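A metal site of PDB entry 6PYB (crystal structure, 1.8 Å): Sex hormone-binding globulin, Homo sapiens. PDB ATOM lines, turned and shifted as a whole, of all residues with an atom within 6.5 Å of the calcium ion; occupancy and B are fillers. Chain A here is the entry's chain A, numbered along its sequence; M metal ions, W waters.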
ATOM      1  N   ASP A  50      -7.809 -14.340  25.300  1.00  0.00           N
ATOM      2  CA  ASP A  50      -8.566 -15.582  25.428  1.00  0.00           C
ATOM      3  C   ASP A  50      -9.864 -15.317  26.170  1.00  0.00           C
ATOM      4  O   ASP A  50      -9.834 -14.768  27.280  1.00  0.00           O
ATOM      5  CB  ASP A  50      -7.735 -16.620  26.163  1.00  0.00           C
ATOM      6  CG  ASP A  50      -8.348 -18.000  26.144  1.00  0.00           C
ATOM      7  OD1 ASP A  50      -9.533 -18.132  25.770  1.00  0.00           O
ATOM      8  OD2 ASP A  50      -7.645 -18.955  26.499  1.00  0.00           O
ATOM      9  N   PRO A  51     -11.030 -15.682  25.617  1.00  0.00           N
ATOM     10  CA  PRO A  51     -12.289 -15.375  26.295  1.00  0.00           C
ATOM     11  C   PRO A  51     -12.690 -16.374  27.383  1.00  0.00           C
ATOM     12  O   PRO A  51     -13.661 -16.104  28.109  1.00  0.00           O
ATOM     13  CB  PRO A  51     -13.310 -15.385  25.148  1.00  0.00           C
ATOM     14  CG  PRO A  51     -12.760 -16.355  24.168  1.00  0.00           C
ATOM     15  CD  PRO A  51     -11.248 -16.252  24.266  1.00  0.00           C
ATOM     16  N   GLU A  52     -11.994 -17.501  27.523  1.00  0.00           N
ATOM     17  CA  GLU A  52     -12.460 -18.550  28.426  1.00  0.00           C
ATOM     18  C   GLU A  52     -11.268 -19.282  29.027  1.00  0.00           C
ATOM     19  O   GLU A  52     -10.316 -19.608  28.325  1.00  0.00           O
ATOM     20  CB  GLU A  52     -13.367 -19.529  27.679  1.00  0.00           C
ATOM     21  CG  GLU A  52     -13.927 -20.629  28.557  1.00  0.00           C
ATOM     22  CD  GLU A  52     -14.979 -21.438  27.832  1.00  0.00           C
ATOM     23  OE1 GLU A  52     -15.875 -20.835  27.199  1.00  0.00           O
ATOM     24  OE2 GLU A  52     -14.923 -22.685  27.899  1.00  0.00           O
ATOM     25  N   GLY A  53     -11.349 -19.549  30.329  1.00  0.00           N
ATOM     26  CA  GLY A  53     -10.332 -20.331  30.984  1.00  0.00           C
ATOM     27  C   GLY A  53     -10.310 -20.066  32.475  1.00  0.00           C
ATOM     28  O   GLY A  53     -11.010 -19.200  32.989  1.00  0.00           O
ATOM     29  N   VAL A 158     -13.688 -24.788  29.363  1.00  0.00           N
ATOM     30  CA  VAL A 158     -12.387 -25.307  28.925  1.00  0.00           C
ATOM     31  C   VAL A 158     -11.312 -24.540  29.687  1.00  0.00           C
ATOM     32  O   VAL A 158     -11.139 -23.335  29.446  1.00  0.00           O
ATOM     33  CB  VAL A 158     -12.205 -25.166  27.402  1.00  0.00           C
ATOM     34  CG1 VAL A 158     -10.865 -25.742  26.984  1.00  0.00           C
ATOM     35  CG2 VAL A 158     -13.337 -25.863  26.673  1.00  0.00           C
ATOM     36  N   PRO A 159     -10.560 -25.190  30.586  1.00  0.00           N
ATOM     37  CA  PRO A 159      -9.765 -24.411  31.553  1.00  0.00           C
ATOM     38  C   PRO A 159      -8.587 -23.654  30.972  1.00  0.00           C
ATOM     39  O   PRO A 159      -8.151 -22.671  31.563  1.00  0.00           O
ATOM     40  CB  PRO A 159      -9.274 -25.482  32.551  1.00  0.00           C
ATOM     41  CG  PRO A 159     -10.066 -26.716  32.256  1.00  0.00           C
ATOM     42  CD  PRO A 159     -10.476 -26.635  30.832  1.00  0.00           C
ATOM     43  N   ALA A 160      -8.042 -24.080  29.828  1.00  0.00           N
ATOM     44  CA  ALA A 160      -6.835 -23.446  29.296  1.00  0.00           C
ATOM     45  C   ALA A 160      -7.067 -21.962  29.067  1.00  0.00           C
ATOM     46  O   ALA A 160      -7.957 -21.569  28.315  1.00  0.00           O
ATOM     47  CB  ALA A 160      -6.425 -24.127  27.985  1.00  0.00           C
ATOM     48  N   LEU A 161      -6.245 -21.137  29.723  1.00  0.00           N
ATOM     49  CA  LEU A 161      -6.328 -19.676  29.613  1.00  0.00           C
ATOM     50  C   LEU A 161      -5.015 -19.164  29.026  1.00  0.00           C
ATOM     51  O   LEU A 161      -4.039 -18.974  29.752  1.00  0.00           O
ATOM     52  CB  LEU A 161      -6.608 -19.032  30.960  1.00  0.00           C
ATOM     53  CG  LEU A 161      -6.856 -17.530  30.919  1.00  0.00           C
ATOM     54  CD1 LEU A 161      -7.990 -17.199  29.963  1.00  0.00           C
ATOM     55  CD2 LEU A 161      -7.149 -16.981  32.301  1.00  0.00           C
ATOM     56  N   ASP A 162      -4.994 -18.934  27.719  1.00  0.00           N
ATOM     57  CA  ASP A 162      -3.800 -18.430  27.056  1.00  0.00           C
ATOM     58  C   ASP A 162      -3.580 -16.967  27.425  1.00  0.00           C
ATOM     59  O   ASP A 162      -4.024 -16.062  26.721  1.00  0.00           O
ATOM     60  CB  ASP A 162      -3.908 -18.604  25.553  1.00  0.00           C
ATOM     61  CG  ASP A 162      -3.973 -20.072  25.140  1.00  0.00           C
ATOM     62  OD1 ASP A 162      -3.059 -20.830  25.529  1.00  0.00           O
ATOM     63  OD2 ASP A 162      -4.926 -20.454  24.444  1.00  0.00           O
HETATM   64 CA    CA M   1      -9.168 -20.605  26.624  1.00  0.00          CA
HETATM   65  O   HOH W   1      -7.580 -21.698  25.046  1.00  0.00           O
HETATM   66  O   HOH W   2     -10.641 -20.551  24.754  1.00  0.00           O
HETATM   67  O   HOH W   3     -10.581 -22.395  26.970  1.00  0.00           O
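The side-chain carboxylate (OD2) of Asp 50 sits close to the backbone NH (N) of Asp 162. OE2 of Glu 52 sits at hydrogen-bond distance from N of Val 158 (2.8 Å).
The calcium ion is bound by OD2 of Asp 50 (2.2 Å), O of Glu 52 (2.3 Å), O of Ala 160 (2.3 Å), water W3 (2.3 Å), water W2 (2.4 Å), water W1 (2.5 Å) and OD1 of Asp 50 (2.6 Å).
The nearest printed residue that does not touch the calcium ion is Leu 161 (4.2 Å).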
